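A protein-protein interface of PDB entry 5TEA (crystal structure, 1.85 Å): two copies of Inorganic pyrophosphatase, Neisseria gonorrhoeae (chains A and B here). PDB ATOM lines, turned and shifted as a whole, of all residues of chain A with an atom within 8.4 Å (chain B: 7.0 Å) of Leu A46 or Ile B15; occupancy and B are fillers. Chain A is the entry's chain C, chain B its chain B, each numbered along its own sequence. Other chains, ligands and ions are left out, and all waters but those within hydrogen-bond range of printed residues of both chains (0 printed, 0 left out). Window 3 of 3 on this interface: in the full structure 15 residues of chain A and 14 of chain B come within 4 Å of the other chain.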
ATOM      1  N   ASP A  11       3.270 -13.201 -19.944  1.00  0.00           N
ATOM      2  CA  ASP A  11       2.880 -14.461 -19.321  1.00  0.00           C
ATOM      3  C   ASP A  11       1.806 -15.149 -20.152  1.00  0.00           C
ATOM      4  O   ASP A  11       0.626 -14.799 -20.087  1.00  0.00           O
ATOM      5  CB  ASP A  11       2.383 -14.237 -17.892  1.00  0.00           C
ATOM      6  CG  ASP A  11       2.073 -15.541 -17.167  1.00  0.00           C
ATOM      7  OD1 ASP A  11       2.260 -16.629 -17.756  1.00  0.00           O
ATOM      8  OD2 ASP A  11       1.641 -15.477 -15.998  1.00  0.00           O
ATOM      9  N   TRP A  42      10.052 -22.519 -21.382  1.00  0.00           N
ATOM     10  CA  TRP A  42       9.342 -21.430 -20.723  1.00  0.00           C
ATOM     11  C   TRP A  42       9.338 -21.676 -19.219  1.00  0.00           C
ATOM     12  O   TRP A  42       8.882 -22.727 -18.758  1.00  0.00           O
ATOM     13  CB  TRP A  42       7.921 -21.347 -21.265  1.00  0.00           C
ATOM     14  CG  TRP A  42       7.012 -20.411 -20.538  1.00  0.00           C
ATOM     15  CD1 TRP A  42       5.983 -20.748 -19.707  1.00  0.00           C
ATOM     16  CD2 TRP A  42       7.037 -18.980 -20.587  1.00  0.00           C
ATOM     17  NE1 TRP A  42       5.369 -19.617 -19.235  1.00  0.00           N
ATOM     18  CE2 TRP A  42       5.992 -18.518 -19.766  1.00  0.00           C
ATOM     19  CE3 TRP A  42       7.840 -18.046 -21.250  1.00  0.00           C
ATOM     20  CZ2 TRP A  42       5.731 -17.161 -19.581  1.00  0.00           C
ATOM     21  CZ3 TRP A  42       7.580 -16.700 -21.066  1.00  0.00           C
ATOM     22  CH2 TRP A  42       6.533 -16.270 -20.242  1.00  0.00           C
ATOM     23  N   ASN A  43       9.872 -20.721 -18.461  1.00  0.00           N
ATOM     24  CA  ASN A  43       9.916 -20.793 -17.001  1.00  0.00           C
ATOM     25  C   ASN A  43       8.656 -20.103 -16.490  1.00  0.00           C
ATOM     26  O   ASN A  43       8.589 -18.872 -16.421  1.00  0.00           O
ATOM     27  CB  ASN A  43      11.200 -20.146 -16.483  1.00  0.00           C
ATOM     28  CG  ASN A  43      11.415 -20.342 -14.989  1.00  0.00           C
ATOM     29  OD1 ASN A  43      10.485 -20.238 -14.194  1.00  0.00           O
ATOM     30  ND2 ASN A  43      12.662 -20.606 -14.602  1.00  0.00           N
ATOM     31  N   ARG A  44       7.638 -20.903 -16.156  1.00  0.00           N
ATOM     32  CA  ARG A  44       6.349 -20.350 -15.753  1.00  0.00           C
ATOM     33  C   ARG A  44       6.478 -19.442 -14.538  1.00  0.00           C
ATOM     34  O   ARG A  44       5.760 -18.442 -14.434  1.00  0.00           O
ATOM     35  CB  ARG A  44       5.360 -21.482 -15.464  1.00  0.00           C
ATOM     36  CG  ARG A  44       3.925 -21.020 -15.246  1.00  0.00           C
ATOM     37  CD  ARG A  44       3.096 -22.065 -14.515  1.00  0.00           C
ATOM     38  NE  ARG A  44       3.576 -23.411 -14.799  1.00  0.00           N
ATOM     39  CZ  ARG A  44       3.141 -24.508 -14.187  1.00  0.00           C
ATOM     40  NH1 ARG A  44       2.201 -24.424 -13.251  1.00  0.00           N
ATOM     41  NH2 ARG A  44       3.648 -25.691 -14.518  1.00  0.00           N
ATOM     42  N   LYS A  45       7.390 -19.763 -13.620  1.00  0.00           N
ATOM     43  CA  LYS A  45       7.562 -18.944 -12.423  1.00  0.00           C
ATOM     44  C   LYS A  45       8.067 -17.549 -12.773  1.00  0.00           C
ATOM     45  O   LYS A  45       7.497 -16.542 -12.336  1.00  0.00           O
ATOM     46  CB  LYS A  45       8.520 -19.636 -11.453  1.00  0.00           C
ATOM     47  N   LEU A  46       9.134 -17.471 -13.565  1.00  0.00           N
ATOM     48  CA  LEU A  46       9.760 -16.204 -13.920  1.00  0.00           C
ATOM     49  C   LEU A  46       9.096 -15.510 -15.102  1.00  0.00           C
ATOM     50  O   LEU A  46       9.366 -14.326 -15.333  1.00  0.00           O
ATOM     51  CB  LEU A  46      11.242 -16.419 -14.245  1.00  0.00           C
ATOM     52  CG  LEU A  46      12.237 -16.679 -13.107  1.00  0.00           C
ATOM     53  CD1 LEU A  46      12.034 -18.034 -12.451  1.00  0.00           C
ATOM     54  CD2 LEU A  46      13.646 -16.570 -13.635  1.00  0.00           C
ATOM     55  N   ALA A  47       8.257 -16.219 -15.860  1.00  0.00           N
ATOM     56  CA  ALA A  47       7.658 -15.691 -17.085  1.00  0.00           C
ATOM     57  C   ALA A  47       8.741 -15.284 -18.083  1.00  0.00           C
ATOM     58  O   ALA A  47       8.733 -14.177 -18.630  1.00  0.00           O
ATOM     59  CB  ALA A  47       6.709 -14.523 -16.788  1.00  0.00           C
ATOM     60  N   ALA A  48       9.686 -16.198 -18.316  1.00  0.00           N
ATOM     61  CA  ALA A  48      10.784 -15.945 -19.239  1.00  0.00           C
ATOM     62  C   ALA A  48      11.279 -17.273 -19.784  1.00  0.00           C
ATOM     63  O   ALA A  48      11.051 -18.324 -19.188  1.00  0.00           O
ATOM     64  CB  ALA A  48      11.930 -15.183 -18.565  1.00  0.00           C
ATOM     65  N   PHE A  49      11.963 -17.213 -20.926  1.00  0.00           N
ATOM     66  CA  PHE A  49      12.515 -18.407 -21.553  1.00  0.00           C
ATOM     67  C   PHE A  49      13.928 -18.664 -21.037  1.00  0.00           C
ATOM     68  O   PHE A  49      14.764 -17.755 -21.016  1.00  0.00           O
ATOM     69  CB  PHE A  49      12.500 -18.267 -23.076  1.00  0.00           C
ATOM     70  CG  PHE A  49      11.115 -18.308 -23.663  1.00  0.00           C
ATOM     71  CD1 PHE A  49      10.495 -19.522 -23.920  1.00  0.00           C
ATOM     72  CD2 PHE A  49      10.432 -17.131 -23.942  1.00  0.00           C
ATOM     73  CE1 PHE A  49       9.209 -19.570 -24.463  1.00  0.00           C
ATOM     74  CE2 PHE A  49       9.140 -17.162 -24.475  1.00  0.00           C
ATOM     75  CZ  PHE A  49       8.531 -18.383 -24.740  1.00  0.00           C
ATOM     76  N   GLN A  50      14.182 -19.899 -20.601  1.00  0.00           N
ATOM     77  CA  GLN A  50      15.454 -20.276 -19.994  1.00  0.00           C
ATOM     78  C   GLN A  50      16.138 -21.318 -20.865  1.00  0.00           C
ATOM     79  O   GLN A  50      15.507 -22.296 -21.275  1.00  0.00           O
ATOM     80  CB  GLN A  50      15.260 -20.832 -18.572  1.00  0.00           C
ATOM     81  CG  GLN A  50      16.551 -21.368 -17.934  1.00  0.00           C
ATOM     82  CD  GLN A  50      16.353 -21.821 -16.496  1.00  0.00           C
ATOM     83  OE1 GLN A  50      15.245 -21.788 -15.972  1.00  0.00           O
ATOM     84  NE2 GLN A  50      17.438 -22.222 -15.849  1.00  0.00           N
ATOM     85  N   ASP B  11      10.879  -8.247 -16.689  1.00  0.00           N
ATOM     86  CA  ASP B  11      11.998  -7.497 -16.125  1.00  0.00           C
ATOM     87  C   ASP B  11      13.001  -8.445 -15.472  1.00  0.00           C
ATOM     88  O   ASP B  11      12.788  -8.926 -14.360  1.00  0.00           O
ATOM     89  CB  ASP B  11      11.499  -6.462 -15.111  1.00  0.00           C
ATOM     90  CG  ASP B  11      12.604  -5.527 -14.631  1.00  0.00           C
ATOM     91  OD1 ASP B  11      13.777  -5.708 -15.031  1.00  0.00           O
ATOM     92  OD2 ASP B  11      12.293  -4.600 -13.851  1.00  0.00           O
ATOM     93  N   PHE B  12      14.109  -8.687 -16.174  1.00  0.00           N
ATOM     94  CA  PHE B  12      15.095  -9.659 -15.712  1.00  0.00           C
ATOM     95  C   PHE B  12      15.773  -9.229 -14.413  1.00  0.00           C
ATOM     96  O   PHE B  12      16.225 -10.086 -13.641  1.00  0.00           O
ATOM     97  CB  PHE B  12      16.136  -9.895 -16.806  1.00  0.00           C
ATOM     98  CG  PHE B  12      15.595 -10.616 -18.008  1.00  0.00           C
ATOM     99  CD1 PHE B  12      15.294 -11.967 -17.941  1.00  0.00           C
ATOM    100  CD2 PHE B  12      15.396  -9.950 -19.208  1.00  0.00           C
ATOM    101  CE1 PHE B  12      14.807 -12.639 -19.039  1.00  0.00           C
ATOM    102  CE2 PHE B  12      14.903 -10.617 -20.314  1.00  0.00           C
ATOM    103  CZ  PHE B  12      14.610 -11.961 -20.229  1.00  0.00           C
ATOM    104  N   ASN B  13      15.861  -7.923 -14.148  1.00  0.00           N
ATOM    105  CA  ASN B  13      16.499  -7.451 -12.924  1.00  0.00           C
ATOM    106  C   ASN B  13      15.598  -7.569 -11.697  1.00  0.00           C
ATOM    107  O   ASN B  13      16.073  -7.342 -10.577  1.00  0.00           O
ATOM    108  CB  ASN B  13      16.966  -5.999 -13.097  1.00  0.00           C
ATOM    109  CG  ASN B  13      18.234  -5.887 -13.942  1.00  0.00           C
ATOM    110  OD1 ASN B  13      19.180  -6.660 -13.771  1.00  0.00           O
ATOM    111  ND2 ASN B  13      18.251  -4.929 -14.864  1.00  0.00           N
ATOM    112  N   GLN B  14      14.322  -7.920 -11.878  1.00  0.00           N
ATOM    113  CA  GLN B  14      13.408  -8.184 -10.772  1.00  0.00           C
ATOM    114  C   GLN B  14      13.113  -9.663 -10.569  1.00  0.00           C
ATOM    115  O   GLN B  14      12.917 -10.090  -9.430  1.00  0.00           O
ATOM    116  CB  GLN B  14      12.086  -7.435 -10.986  1.00  0.00           C
ATOM    117  N   ILE B  15      13.088 -10.453 -11.641  1.00  0.00           N
ATOM    118  CA  ILE B  15      12.793 -11.877 -11.528  1.00  0.00           C
ATOM    119  C   ILE B  15      14.048 -12.697 -11.243  1.00  0.00           C
ATOM    120  O   ILE B  15      13.964 -13.754 -10.610  1.00  0.00           O
ATOM    121  CB  ILE B  15      12.101 -12.385 -12.806  1.00  0.00           C
ATOM    122  CG1 ILE B  15      13.016 -12.175 -14.018  1.00  0.00           C
ATOM    123  CG2 ILE B  15      10.762 -11.688 -13.009  1.00  0.00           C
ATOM    124  CD1 ILE B  15      12.705 -13.074 -15.195  1.00  0.00           C
ATOM    125  N   LEU B  16      15.206 -12.238 -11.699  1.00  0.00           N
ATOM    126  CA  LEU B  16      16.448 -12.984 -11.595  1.00  0.00           C
ATOM    127  C   LEU B  16      17.394 -12.291 -10.632  1.00  0.00           C
ATOM    128  O   LEU B  16      17.504 -11.060 -10.628  1.00  0.00           O
ATOM    129  CB  LEU B  16      17.141 -13.107 -12.955  1.00  0.00           C
ATOM    130  CG  LEU B  16      16.736 -14.216 -13.914  1.00  0.00           C
ATOM    131  CD1 LEU B  16      17.459 -14.034 -15.258  1.00  0.00           C
ATOM    132  CD2 LEU B  16      17.047 -15.561 -13.296  1.00  0.00           C
ATOM    133  N   THR B  17      18.086 -13.084  -9.842  1.00  0.00           N
ATOM    134  CA  THR B  17      19.209 -12.646  -9.036  1.00  0.00           C
ATOM    135  C   THR B  17      20.506 -13.013  -9.736  1.00  0.00           C
ATOM    136  O   THR B  17      20.498 -13.703 -10.761  1.00  0.00           O
ATOM    137  CB  THR B  17      19.142 -13.299  -7.659  1.00  0.00           C
ATOM    138  OG1 THR B  17      19.378 -14.704  -7.797  1.00  0.00           O
ATOM    139  CG2 THR B  17      17.784 -13.061  -7.027  1.00  0.00           C
ATOM    140  N   ASN B  27      23.554 -16.453 -12.982  1.00  0.00           N
ATOM    141  CA  ASN B  27      22.509 -16.252 -13.981  1.00  0.00           C
ATOM    142  C   ASN B  27      22.979 -15.211 -14.987  1.00  0.00           C
ATOM    143  O   ASN B  27      23.497 -14.159 -14.598  1.00  0.00           O
ATOM    144  CB  ASN B  27      21.192 -15.817 -13.324  1.00  0.00           C
ATOM    145  CG  ASN B  27      20.614 -16.890 -12.411  1.00  0.00           C
ATOM    146  OD1 ASN B  27      20.708 -18.074 -12.707  1.00  0.00           O
ATOM    147  ND2 ASN B  27      20.037 -16.477 -11.290  1.00  0.00           N
ATOM    148  N   PRO B  69      22.181 -10.121 -14.106  1.00  0.00           N
ATOM    149  CA  PRO B  69      21.146  -9.290 -13.472  1.00  0.00           C
ATOM    150  C   PRO B  69      21.584  -8.802 -12.097  1.00  0.00           C
ATOM    151  O   PRO B  69      22.334  -9.474 -11.388  1.00  0.00           O
ATOM    152  CB  PRO B  69      19.935 -10.232 -13.357  1.00  0.00           C
ATOM    153  CG  PRO B  69      20.275 -11.461 -14.123  1.00  0.00           C
ATOM    154  CD  PRO B  69      21.759 -11.519 -14.301  1.00  0.00           C
ATOM    155  N   GLN B  70      21.107  -7.606 -11.738  1.00  0.00           N
ATOM    156  CA  GLN B  70      21.292  -7.029 -10.401  1.00  0.00           C
ATOM    157  C   GLN B  70      22.767  -6.811 -10.075  1.00  0.00           C
ATOM    158  O   GLN B  70      23.214  -7.045  -8.954  1.00  0.00           O
ATOM    159  CB  GLN B  70      20.613  -7.878  -9.324  1.00  0.00           C
ATOM    160  CG  GLN B  70      19.123  -8.035  -9.543  1.00  0.00           C
ATOM    161  CD  GLN B  70      18.424  -8.691  -8.371  1.00  0.00           C
ATOM    162  OE1 GLN B  70      19.063  -9.255  -7.482  1.00  0.00           O
ATOM    163  NE2 GLN B  70      17.100  -8.616  -8.360  1.00  0.00           N
ATOM    164  N   PHE B  94      17.744 -16.477 -20.893  1.00  0.00           N
ATOM    165  CA  PHE B  94      18.665 -16.474 -19.769  1.00  0.00           C
ATOM    166  C   PHE B  94      19.063 -17.910 -19.455  1.00  0.00           C
ATOM    167  O   PHE B  94      18.396 -18.860 -19.869  1.00  0.00           O
ATOM    168  CB  PHE B  94      18.060 -15.791 -18.541  1.00  0.00           C
ATOM    169  CG  PHE B  94      17.097 -16.657 -17.766  1.00  0.00           C
ATOM    170  CD1 PHE B  94      15.756 -16.719 -18.123  1.00  0.00           C
ATOM    171  CD2 PHE B  94      17.528 -17.398 -16.680  1.00  0.00           C
ATOM    172  CE1 PHE B  94      14.864 -17.513 -17.412  1.00  0.00           C
ATOM    173  CE2 PHE B  94      16.637 -18.207 -15.972  1.00  0.00           C
ATOM    174  CZ  PHE B  94      15.310 -18.250 -16.334  1.00  0.00           C
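The side-chain amide oxygen (OD1) of Asn A43 sits close to the backbone NH (N) of Lys A45 (3.2 Å). The side-chain amide nitrogen (ND2) of Asn A43 is in hydrogen-bond range of the side-chain amide oxygen (OE1) of Gln A50, at 3.2 Å. The backbone carbonyl oxygen (O) of Ala A48 is in hydrogen-bond range of the backbone NH (N) of Asn A43, at 2.8 Å. N of Leu A46 is in hydrogen-bond range of OD1 of Asn A43 (3.1 Å). NE2 of Gln B70 is in hydrogen-bond range of O of Leu B16 (3.4 Å).
Leu A46 touches just these residues of chain B: Ile B15 (3.6 Å), Leu B16 (3.6 Å) and Phe B94 (3.6 Å). Ile B15 touches one residue of chain A. No residue of chain A comes within 4 Å of Gln B14. Printed residues of chain B within 4 Å of Phe A49: Phe B94 (3.2 Å). Of the printed residues of chain A, Leu B16 touches Leu A46 (3.6 Å). Pro B69 touches none of the printed residues of chain A. The nearest residue of chain B that does not touch Leu A46 is Asp B11 (6.4 Å). The nearest residue of chain A that does not touch Ile B15 is Ala A48 (4.1 Å).
N of Phe B94 sits close to O of Phe A49 (3.2 Å).
Hydrophobic or aromatic side chains of chain B that line the printed part of chain A: Phe B12, Ile B15, Leu B16 and Phe B94.
ND2 of Asn A43 touches CZ of Phe B94 (3.9 Å). CD1 of Ile B15 touches O of Leu A46 (3.6 Å). Leu A46 touches Leu B16. CD2 of Leu A46 touches CZ of Phe B94, at 3.6 Å. CE1 of Phe B12 touches CB of Ala A48, at 3.9 Å. Phe B94 touches Ala A48. Gln A50 touches Phe B94 (CA to O, 3.3 Å).
1 position is printed for both chains. Of the 8 pairs that touch across the chains among the printed residues, none has its exchanged pair printed and touching as well.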
